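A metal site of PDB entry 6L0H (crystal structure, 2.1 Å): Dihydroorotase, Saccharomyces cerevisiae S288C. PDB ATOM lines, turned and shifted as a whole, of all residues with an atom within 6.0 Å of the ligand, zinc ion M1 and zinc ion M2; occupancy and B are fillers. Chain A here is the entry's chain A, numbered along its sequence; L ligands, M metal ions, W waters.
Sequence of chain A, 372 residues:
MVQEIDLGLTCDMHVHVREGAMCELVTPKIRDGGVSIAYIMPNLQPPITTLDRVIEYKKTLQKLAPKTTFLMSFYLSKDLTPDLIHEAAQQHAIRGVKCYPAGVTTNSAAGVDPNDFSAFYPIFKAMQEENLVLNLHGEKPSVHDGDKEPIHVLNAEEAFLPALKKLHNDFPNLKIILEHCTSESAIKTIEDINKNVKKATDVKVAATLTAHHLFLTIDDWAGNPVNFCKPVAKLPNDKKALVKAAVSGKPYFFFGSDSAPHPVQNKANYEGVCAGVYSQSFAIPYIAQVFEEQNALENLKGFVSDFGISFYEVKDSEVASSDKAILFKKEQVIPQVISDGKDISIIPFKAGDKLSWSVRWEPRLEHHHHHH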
ATOM      1  N   HIS A  14      -8.634   7.391   8.374  1.00  0.00           N
ATOM      2  CA  HIS A  14      -9.421   6.329   7.718  1.00  0.00           C
ATOM      3  C   HIS A  14      -8.824   4.976   8.130  1.00  0.00           C
ATOM      4  O   HIS A  14      -7.898   4.492   7.487  1.00  0.00           O
ATOM      5  CB  HIS A  14      -9.441   6.530   6.221  1.00  0.00           C
ATOM      6  CG  HIS A  14     -10.421   5.665   5.504  1.00  0.00           C
ATOM      7  ND1 HIS A  14     -11.209   6.128   4.466  1.00  0.00           N
ATOM      8  CD2 HIS A  14     -10.730   4.354   5.647  1.00  0.00           C
ATOM      9  CE1 HIS A  14     -11.957   5.133   4.017  1.00  0.00           C
ATOM     10  NE2 HIS A  14     -11.681   4.047   4.722  1.00  0.00           N
ATOM     11  N   HIS A  16      -9.515   0.887   9.574  1.00  0.00           N
ATOM     12  CA  HIS A  16     -10.302  -0.312   9.864  1.00  0.00           C
ATOM     13  C   HIS A  16      -9.552  -1.149  10.885  1.00  0.00           C
ATOM     14  O   HIS A  16      -8.382  -1.480  10.684  1.00  0.00           O
ATOM     15  CB  HIS A  16     -10.570  -1.138   8.606  1.00  0.00           C
ATOM     16  CG  HIS A  16     -11.366  -0.391   7.590  1.00  0.00           C
ATOM     17  ND1 HIS A  16     -12.736  -0.359   7.611  1.00  0.00           N
ATOM     18  CD2 HIS A  16     -10.982   0.378   6.548  1.00  0.00           C
ATOM     19  CE1 HIS A  16     -13.173   0.392   6.611  1.00  0.00           C
ATOM     20  NE2 HIS A  16     -12.121   0.863   5.956  1.00  0.00           N
ATOM     21  N   ARG A  18     -11.524  -3.833  12.699  1.00  0.00           N
ATOM     22  CA  ARG A  18     -12.285  -5.089  12.824  1.00  0.00           C
ATOM     23  C   ARG A  18     -12.711  -5.320  14.281  1.00  0.00           C
ATOM     24  O   ARG A  18     -12.890  -4.371  15.054  1.00  0.00           O
ATOM     25  CB  ARG A  18     -11.489  -6.256  12.234  1.00  0.00           C
ATOM     26  CG  ARG A  18     -10.827  -6.006  10.888  1.00  0.00           C
ATOM     27  CD  ARG A  18     -11.795  -5.566   9.805  1.00  0.00           C
ATOM     28  NE  ARG A  18     -11.084  -5.554   8.526  1.00  0.00           N
ATOM     29  CZ  ARG A  18     -11.481  -4.910   7.434  1.00  0.00           C
ATOM     30  NH1 ARG A  18     -12.624  -4.190   7.428  1.00  0.00           N
ATOM     31  NH2 ARG A  18     -10.745  -5.000   6.336  1.00  0.00           N
ATOM     32  N   MET A  41     -13.499   3.505  11.142  1.00  0.00           N
ATOM     33  CA  MET A  41     -14.599   3.244  10.223  1.00  0.00           C
ATOM     34  C   MET A  41     -15.553   2.201  10.790  1.00  0.00           C
ATOM     35  O   MET A  41     -15.167   1.364  11.614  1.00  0.00           O
ATOM     36  CB  MET A  41     -14.061   2.818   8.864  1.00  0.00           C
ATOM     37  CG  MET A  41     -13.490   3.979   8.074  1.00  0.00           C
ATOM     38  SD  MET A  41     -14.618   5.422   7.933  1.00  0.00           S
ATOM     39  CE  MET A  41     -13.562   6.635   7.125  1.00  0.00           C
ATOM     40  N   ASN A  43     -17.763  -0.252   9.320  1.00  0.00           N
ATOM     41  CA  ASN A  43     -18.322  -1.388   8.575  1.00  0.00           C
ATOM     42  C   ASN A  43     -17.983  -2.727   9.247  1.00  0.00           C
ATOM     43  O   ASN A  43     -17.332  -3.601   8.670  1.00  0.00           O
ATOM     44  CB  ASN A  43     -17.846  -1.356   7.135  1.00  0.00           C
ATOM     45  CG  ASN A  43     -16.349  -1.509   7.023  1.00  0.00           C
ATOM     46  OD1 ASN A  43     -15.605  -1.172   7.947  1.00  0.00           O
ATOM     47  ND2 ASN A  43     -15.887  -2.027   5.874  1.00  0.00           N
ATOM     48  N   KCX A  98     -20.390   7.431   8.058  1.00  0.00           N
ATOM     49  CA  KCX A  98     -19.708   6.957   6.860  1.00  0.00           C
ATOM     50  CB  KCX A  98     -18.597   5.959   7.242  1.00  0.00           C
ATOM     51  CG  KCX A  98     -17.994   5.214   6.055  1.00  0.00           C
ATOM     52  CD  KCX A  98     -17.196   6.171   5.164  1.00  0.00           C
ATOM     53  CE  KCX A  98     -16.383   5.425   4.117  1.00  0.00           C
ATOM     54  NZ  KCX A  98     -15.631   4.338   4.771  1.00  0.00           N
ATOM     55  C   KCX A  98     -20.687   6.309   5.903  1.00  0.00           C
ATOM     56  O   KCX A  98     -21.467   5.438   6.294  1.00  0.00           O
ATOM     57  CX  KCX A  98     -14.806   3.547   4.076  1.00  0.00           C
ATOM     58  OQ1 KCX A  98     -14.208   2.627   4.658  1.00  0.00           O
ATOM     59  OQ2 KCX A  98     -14.654   3.746   2.859  1.00  0.00           O
ATOM     60  N   TYR A 100     -21.409   3.938   2.738  1.00  0.00           N
ATOM     61  CA  TYR A 100     -20.968   2.893   1.806  1.00  0.00           C
ATOM     62  C   TYR A 100     -22.063   2.673   0.779  1.00  0.00           C
ATOM     63  O   TYR A 100     -23.169   2.277   1.167  1.00  0.00           O
ATOM     64  CB  TYR A 100     -20.662   1.577   2.528  1.00  0.00           C
ATOM     65  CG  TYR A 100     -19.489   1.620   3.486  1.00  0.00           C
ATOM     66  CD1 TYR A 100     -18.198   1.359   3.044  1.00  0.00           C
ATOM     67  CD2 TYR A 100     -19.671   1.914   4.820  1.00  0.00           C
ATOM     68  CE1 TYR A 100     -17.134   1.396   3.898  1.00  0.00           C
ATOM     69  CE2 TYR A 100     -18.604   1.938   5.705  1.00  0.00           C
ATOM     70  CZ  TYR A 100     -17.330   1.686   5.213  1.00  0.00           C
ATOM     71  OH  TYR A 100     -16.246   1.716   6.059  1.00  0.00           O
ATOM     72  N   VAL A 104     -20.241  -2.239  -3.165  1.00  0.00           N
ATOM     73  CA  VAL A 104     -18.970  -1.833  -3.786  1.00  0.00           C
ATOM     74  C   VAL A 104     -17.732  -2.211  -2.977  1.00  0.00           C
ATOM     75  O   VAL A 104     -16.620  -2.106  -3.524  1.00  0.00           O
ATOM     76  CB  VAL A 104     -18.900  -0.325  -4.115  1.00  0.00           C
ATOM     77  CG1 VAL A 104     -20.062   0.077  -5.014  1.00  0.00           C
ATOM     78  CG2 VAL A 104     -18.860   0.535  -2.827  1.00  0.00           C
ATOM     79  N   THR A 105     -17.866  -2.623  -1.703  1.00  0.00           N
ATOM     80  CA  THR A 105     -16.669  -2.991  -0.928  1.00  0.00           C
ATOM     81  C   THR A 105     -17.057  -3.837   0.287  1.00  0.00           C
ATOM     82  O   THR A 105     -18.216  -4.230   0.464  1.00  0.00           O
ATOM     83  CB  THR A 105     -15.856  -1.768  -0.496  1.00  0.00           C
ATOM     84  OG1 THR A 105     -14.597  -2.198   0.003  1.00  0.00           O
ATOM     85  CG2 THR A 105     -16.588  -0.949   0.574  1.00  0.00           C
ATOM     86  N   THR A 106     -16.059  -4.107   1.151  1.00  0.00           N
ATOM     87  CA  THR A 106     -16.253  -4.948   2.332  1.00  0.00           C
ATOM     88  C   THR A 106     -17.432  -4.481   3.196  1.00  0.00           C
ATOM     89  O   THR A 106     -17.506  -3.324   3.606  1.00  0.00           O
ATOM     90  CB  THR A 106     -14.973  -4.964   3.190  1.00  0.00           C
ATOM     91  OG1 THR A 106     -13.870  -5.472   2.420  1.00  0.00           O
ATOM     92  CG2 THR A 106     -15.144  -5.840   4.433  1.00  0.00           C
ATOM     93  N   HIS A 137     -17.515   6.836   0.767  1.00  0.00           N
ATOM     94  CA  HIS A 137     -16.838   5.917  -0.151  1.00  0.00           C
ATOM     95  C   HIS A 137     -17.466   6.212  -1.500  1.00  0.00           C
ATOM     96  O   HIS A 137     -18.498   5.648  -1.875  1.00  0.00           O
ATOM     97  CB  HIS A 137     -16.990   4.451   0.242  1.00  0.00           C
ATOM     98  CG  HIS A 137     -16.253   3.499  -0.647  1.00  0.00           C
ATOM     99  ND1 HIS A 137     -15.270   2.637  -0.191  1.00  0.00           N
ATOM    100  CD2 HIS A 137     -16.353   3.284  -1.984  1.00  0.00           C
ATOM    101  CE1 HIS A 137     -14.792   1.944  -1.202  1.00  0.00           C
ATOM    102  NE2 HIS A 137     -15.427   2.309  -2.310  1.00  0.00           N
ATOM    103  N   GLU A 179     -13.474  10.037   0.631  1.00  0.00           N
ATOM    104  CA  GLU A 179     -12.425   9.188   1.180  1.00  0.00           C
ATOM    105  C   GLU A 179     -11.594   8.559   0.060  1.00  0.00           C
ATOM    106  O   GLU A 179     -12.051   8.423  -1.078  1.00  0.00           O
ATOM    107  CB  GLU A 179     -13.050   8.093   2.072  1.00  0.00           C
ATOM    108  CG  GLU A 179     -13.763   8.613   3.344  1.00  0.00           C
ATOM    109  CD  GLU A 179     -12.808   9.263   4.353  1.00  0.00           C
ATOM    110  OE1 GLU A 179     -11.601   8.957   4.323  1.00  0.00           O
ATOM    111  OE2 GLU A 179     -13.251  10.062   5.220  1.00  0.00           O
ATOM    112  N   HIS A 180     -10.347   8.216   0.387  1.00  0.00           N
ATOM    113  CA  HIS A 180      -9.372   7.524  -0.462  1.00  0.00           C
ATOM    114  C   HIS A 180      -9.562   7.775  -1.959  1.00  0.00           C
ATOM    115  O   HIS A 180      -9.978   6.881  -2.708  1.00  0.00           O
ATOM    116  CB  HIS A 180      -9.364   6.008  -0.168  1.00  0.00           C
ATOM    117  CG  HIS A 180     -10.720   5.379  -0.077  1.00  0.00           C
ATOM    118  ND1 HIS A 180     -11.730   5.630  -0.979  1.00  0.00           N
ATOM    119  CD2 HIS A 180     -11.238   4.489   0.812  1.00  0.00           C
ATOM    120  CE1 HIS A 180     -12.814   4.931  -0.655  1.00  0.00           C
ATOM    121  NE2 HIS A 180     -12.536   4.232   0.422  1.00  0.00           N
ATOM    122  N   CYS A 229      -7.763  -3.623  -3.661  1.00  0.00           N
ATOM    123  CA  CYS A 229      -8.545  -2.850  -2.707  1.00  0.00           C
ATOM    124  C   CYS A 229      -9.613  -2.074  -3.472  1.00  0.00           C
ATOM    125  O   CYS A 229      -9.640  -2.080  -4.702  1.00  0.00           O
ATOM    126  CB  CYS A 229      -7.646  -1.887  -1.907  1.00  0.00           C
ATOM    127  SG  CYS A 229      -6.892  -0.615  -2.964  1.00  0.00           S
ATOM    128  N   LYS A 230     -10.533  -1.466  -2.722  1.00  0.00           N
ATOM    129  CA  LYS A 230     -11.517  -0.517  -3.252  1.00  0.00           C
ATOM    130  C   LYS A 230     -11.269   0.888  -2.692  1.00  0.00           C
ATOM    131  O   LYS A 230     -10.979   1.025  -1.495  1.00  0.00           O
ATOM    132  CB  LYS A 230     -12.941  -0.946  -2.893  1.00  0.00           C
ATOM    133  CG  LYS A 230     -13.342  -2.275  -3.481  1.00  0.00           C
ATOM    134  CD  LYS A 230     -13.049  -2.290  -4.969  1.00  0.00           C
ATOM    135  CE  LYS A 230     -14.226  -2.759  -5.743  1.00  0.00           C
ATOM    136  NZ  LYS A 230     -15.169  -1.685  -6.140  1.00  0.00           N
ATOM    137  N   PRO A 231     -11.371   1.964  -3.505  1.00  0.00           N
ATOM    138  CA  PRO A 231     -11.444   1.916  -4.968  1.00  0.00           C
ATOM    139  C   PRO A 231     -10.148   1.307  -5.493  1.00  0.00           C
ATOM    140  O   PRO A 231      -9.098   1.389  -4.848  1.00  0.00           O
ATOM    141  CB  PRO A 231     -11.595   3.389  -5.399  1.00  0.00           C
ATOM    142  CG  PRO A 231     -11.858   4.166  -4.127  1.00  0.00           C
ATOM    143  CD  PRO A 231     -11.232   3.343  -3.024  1.00  0.00           C
ATOM    144  N   ASP A 258      -6.849   3.991   4.919  1.00  0.00           N
ATOM    145  CA  ASP A 258      -7.754   2.869   4.630  1.00  0.00           C
ATOM    146  C   ASP A 258      -7.032   1.536   4.811  1.00  0.00           C
ATOM    147  O   ASP A 258      -7.238   0.562   4.049  1.00  0.00           O
ATOM    148  CB  ASP A 258      -8.378   2.964   3.244  1.00  0.00           C
ATOM    149  CG  ASP A 258      -9.531   1.958   3.058  1.00  0.00           C
ATOM    150  OD1 ASP A 258     -10.202   1.647   4.054  1.00  0.00           O
ATOM    151  OD2 ASP A 258      -9.750   1.472   1.924  1.00  0.00           O
ATOM    152  N   ALA A 260      -6.883  -1.848   5.866  1.00  0.00           N
ATOM    153  CA  ALA A 260      -8.035  -2.734   5.904  1.00  0.00           C
ATOM    154  C   ALA A 260      -7.512  -4.154   6.083  1.00  0.00           C
ATOM    155  O   ALA A 260      -7.224  -4.847   5.096  1.00  0.00           O
ATOM    156  CB  ALA A 260      -8.864  -2.584   4.628  1.00  0.00           C
ATOM    157  N   PRO A 261      -7.332  -4.613   7.329  1.00  0.00           N
ATOM    158  CA  PRO A 261      -6.719  -5.929   7.539  1.00  0.00           C
ATOM    159  C   PRO A 261      -7.662  -7.076   7.222  1.00  0.00           C
ATOM    160  O   PRO A 261      -8.856  -7.020   7.503  1.00  0.00           O
ATOM    161  CB  PRO A 261      -6.303  -5.921   9.012  1.00  0.00           C
ATOM    162  CG  PRO A 261      -6.964  -4.710   9.640  1.00  0.00           C
ATOM    163  CD  PRO A 261      -7.639  -3.905   8.581  1.00  0.00           C
ATOM    164  N   HIS A 262      -7.122  -8.107   6.552  1.00  0.00           N
ATOM    165  CA  HIS A 262      -7.781  -9.383   6.282  1.00  0.00           C
ATOM    166  C   HIS A 262      -6.781 -10.500   6.579  1.00  0.00           C
ATOM    167  O   HIS A 262      -5.600 -10.394   6.192  1.00  0.00           O
ATOM    168  CB  HIS A 262      -8.236  -9.525   4.828  1.00  0.00           C
ATOM    169  CG  HIS A 262      -9.231  -8.497   4.387  1.00  0.00           C
ATOM    170  ND1 HIS A 262     -10.557  -8.533   4.783  1.00  0.00           N
ATOM    171  CD2 HIS A 262      -9.102  -7.414   3.579  1.00  0.00           C
ATOM    172  CE1 HIS A 262     -11.198  -7.511   4.230  1.00  0.00           C
ATOM    173  NE2 HIS A 262     -10.337  -6.822   3.504  1.00  0.00           N
ATOM    174  N   ALA A 275     -11.373  -7.283  -0.537  1.00  0.00           N
ATOM    175  CA  ALA A 275     -10.681  -6.049  -0.904  1.00  0.00           C
ATOM    176  C   ALA A 275     -10.081  -5.390   0.338  1.00  0.00           C
ATOM    177  O   ALA A 275     -10.752  -5.238   1.362  1.00  0.00           O
ATOM    178  CB  ALA A 275     -11.638  -5.080  -1.605  1.00  0.00           C
ATOM    179  N   GLY A 276      -8.829  -4.960   0.241  1.00  0.00           N
ATOM    180  CA  GLY A 276      -8.180  -4.249   1.325  1.00  0.00           C
ATOM    181  C   GLY A 276      -6.688  -4.515   1.413  1.00  0.00           C
ATOM    182  O   GLY A 276      -6.219  -5.642   1.192  1.00  0.00           O
HETATM  183  C1  LIG L   1     -12.474  -3.021   4.124  1.00  0.00           C
HETATM  184  O1  LIG L   1     -12.114  -4.207   3.938  1.00  0.00           O
HETATM  185  O2  LIG L   1     -13.137  -2.671   5.141  1.00  0.00           O
HETATM  186  C2  LIG L   1     -12.114  -1.974   3.071  1.00  0.00           C
HETATM  187  O3  LIG L   1     -11.944  -2.636   1.852  1.00  0.00           O
HETATM  188  C3  LIG L   1     -13.305  -1.035   3.060  1.00  0.00           C
HETATM  189  C4  LIG L   1     -13.035   0.155   2.149  1.00  0.00           C
HETATM  190  O4  LIG L   1     -13.308   0.044   0.925  1.00  0.00           O
HETATM  191  O5  LIG L   1     -12.581   1.230   2.640  1.00  0.00           O
HETATM  192 ZN    ZN M   1     -13.797   2.756   1.296  1.00  0.00          ZN
HETATM  193 ZN    ZN M   2     -12.117   2.097   4.319  1.00  0.00          ZN
HETATM  194  O   HOH W   1     -10.152  -1.300   0.234  1.00  0.00           O
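A ring nitrogen (ND1) of His 14 lies within hydrogen-bond range of the side-chain carboxylate (OE1) of Glu 179.
NZ of KCX 98 lies within hydrogen-bond range of the side-chain sulfur (SD) of Met 41 (3.5 Å).
NZ of KCX 98 sits at hydrogen-bond distance from the side-chain hydroxyl (OH) of Tyr 100 (3.0 Å).
ND1 of His 16 sits at hydrogen-bond distance from OD1 of Asn 43.
The backbone carbonyl oxygen of Thr 106 is in hydrogen-bond range of the side-chain amide nitrogen of Asn 43, at 3.1 Å.
NH2 of Arg 18 sits close to NE2 of His 262, 3.4 Å away.
The backbone carbonyl oxygen of Pro 261 sits at hydrogen-bond distance from the guanidinium group of Arg 18 (2.9 Å).
The side-chain amino group (NZ) of Lys 230 is in hydrogen-bond range of the backbone carbonyl oxygen (O) of Val 104 (3.0 Å).
Zinc ion M1 is bound by OQ2 of KCX 98 (2.0 Å), ND1 of His 137 (2.1 Å), NE2 of His 180 (2.1 Å) and O5 of the ligand (2.4 Å).
Slightly farther from zinc ion M1 lies O4 of the ligand (2.8 Å).
Zinc ion M2 is bound by an oxygen (O5) of the ligand, the side-chain carboxylate (OD1) of Asp 258, a ring nitrogen (NE2) of His 14, a ring nitrogen (NE2) of His 16 and OQ1 of KCX 98.
Within 4 Å of zinc ion M1: KCX 98, His 137 and His 180.
The backbone carbonyl oxygen (O) of Lys 230 sits close to an oxygen (O4) of the ligand (3.5 Å).
Merely in contact with the ligand: Ala 260.
Along chain A the residues within 4 Å of the ligand span positions 14 to 275.
The nearest printed residue that does not touch the ligand is Gly 276 (4.1 Å).
Water W1 lies within hydrogen-bond range of an oxygen (O3) of the ligand, the backbone NH of Lys 230 and the side-chain carboxylate of Asp 258.
The side-chain hydroxyl of Thr 106 lies within hydrogen-bond range of an oxygen (O1) of the ligand (2.6 Å).
An oxygen (O4) of the ligand sits at hydrogen-bond distance from the side-chain hydroxyl (OG1) of Thr 105.
The guanidinium group (NH1) of Arg 18 lies within salt-bridge range of an oxygen (O2) of the ligand (2.8 Å).
The backbone carbonyl oxygen of Ala 275 sits at hydrogen-bond distance from an oxygen (O3) of the ligand (2.9 Å).
The side-chain amide nitrogen (ND2) of Asn 43 sits at hydrogen-bond distance from an oxygen (O2) of the ligand (2.9 Å).
A ring nitrogen (NE2) of His 262 lies within hydrogen-bond range of an oxygen (O1) of the ligand.
The nearest printed residue that does not touch zinc ion M2 is His 180 (4.3 Å).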
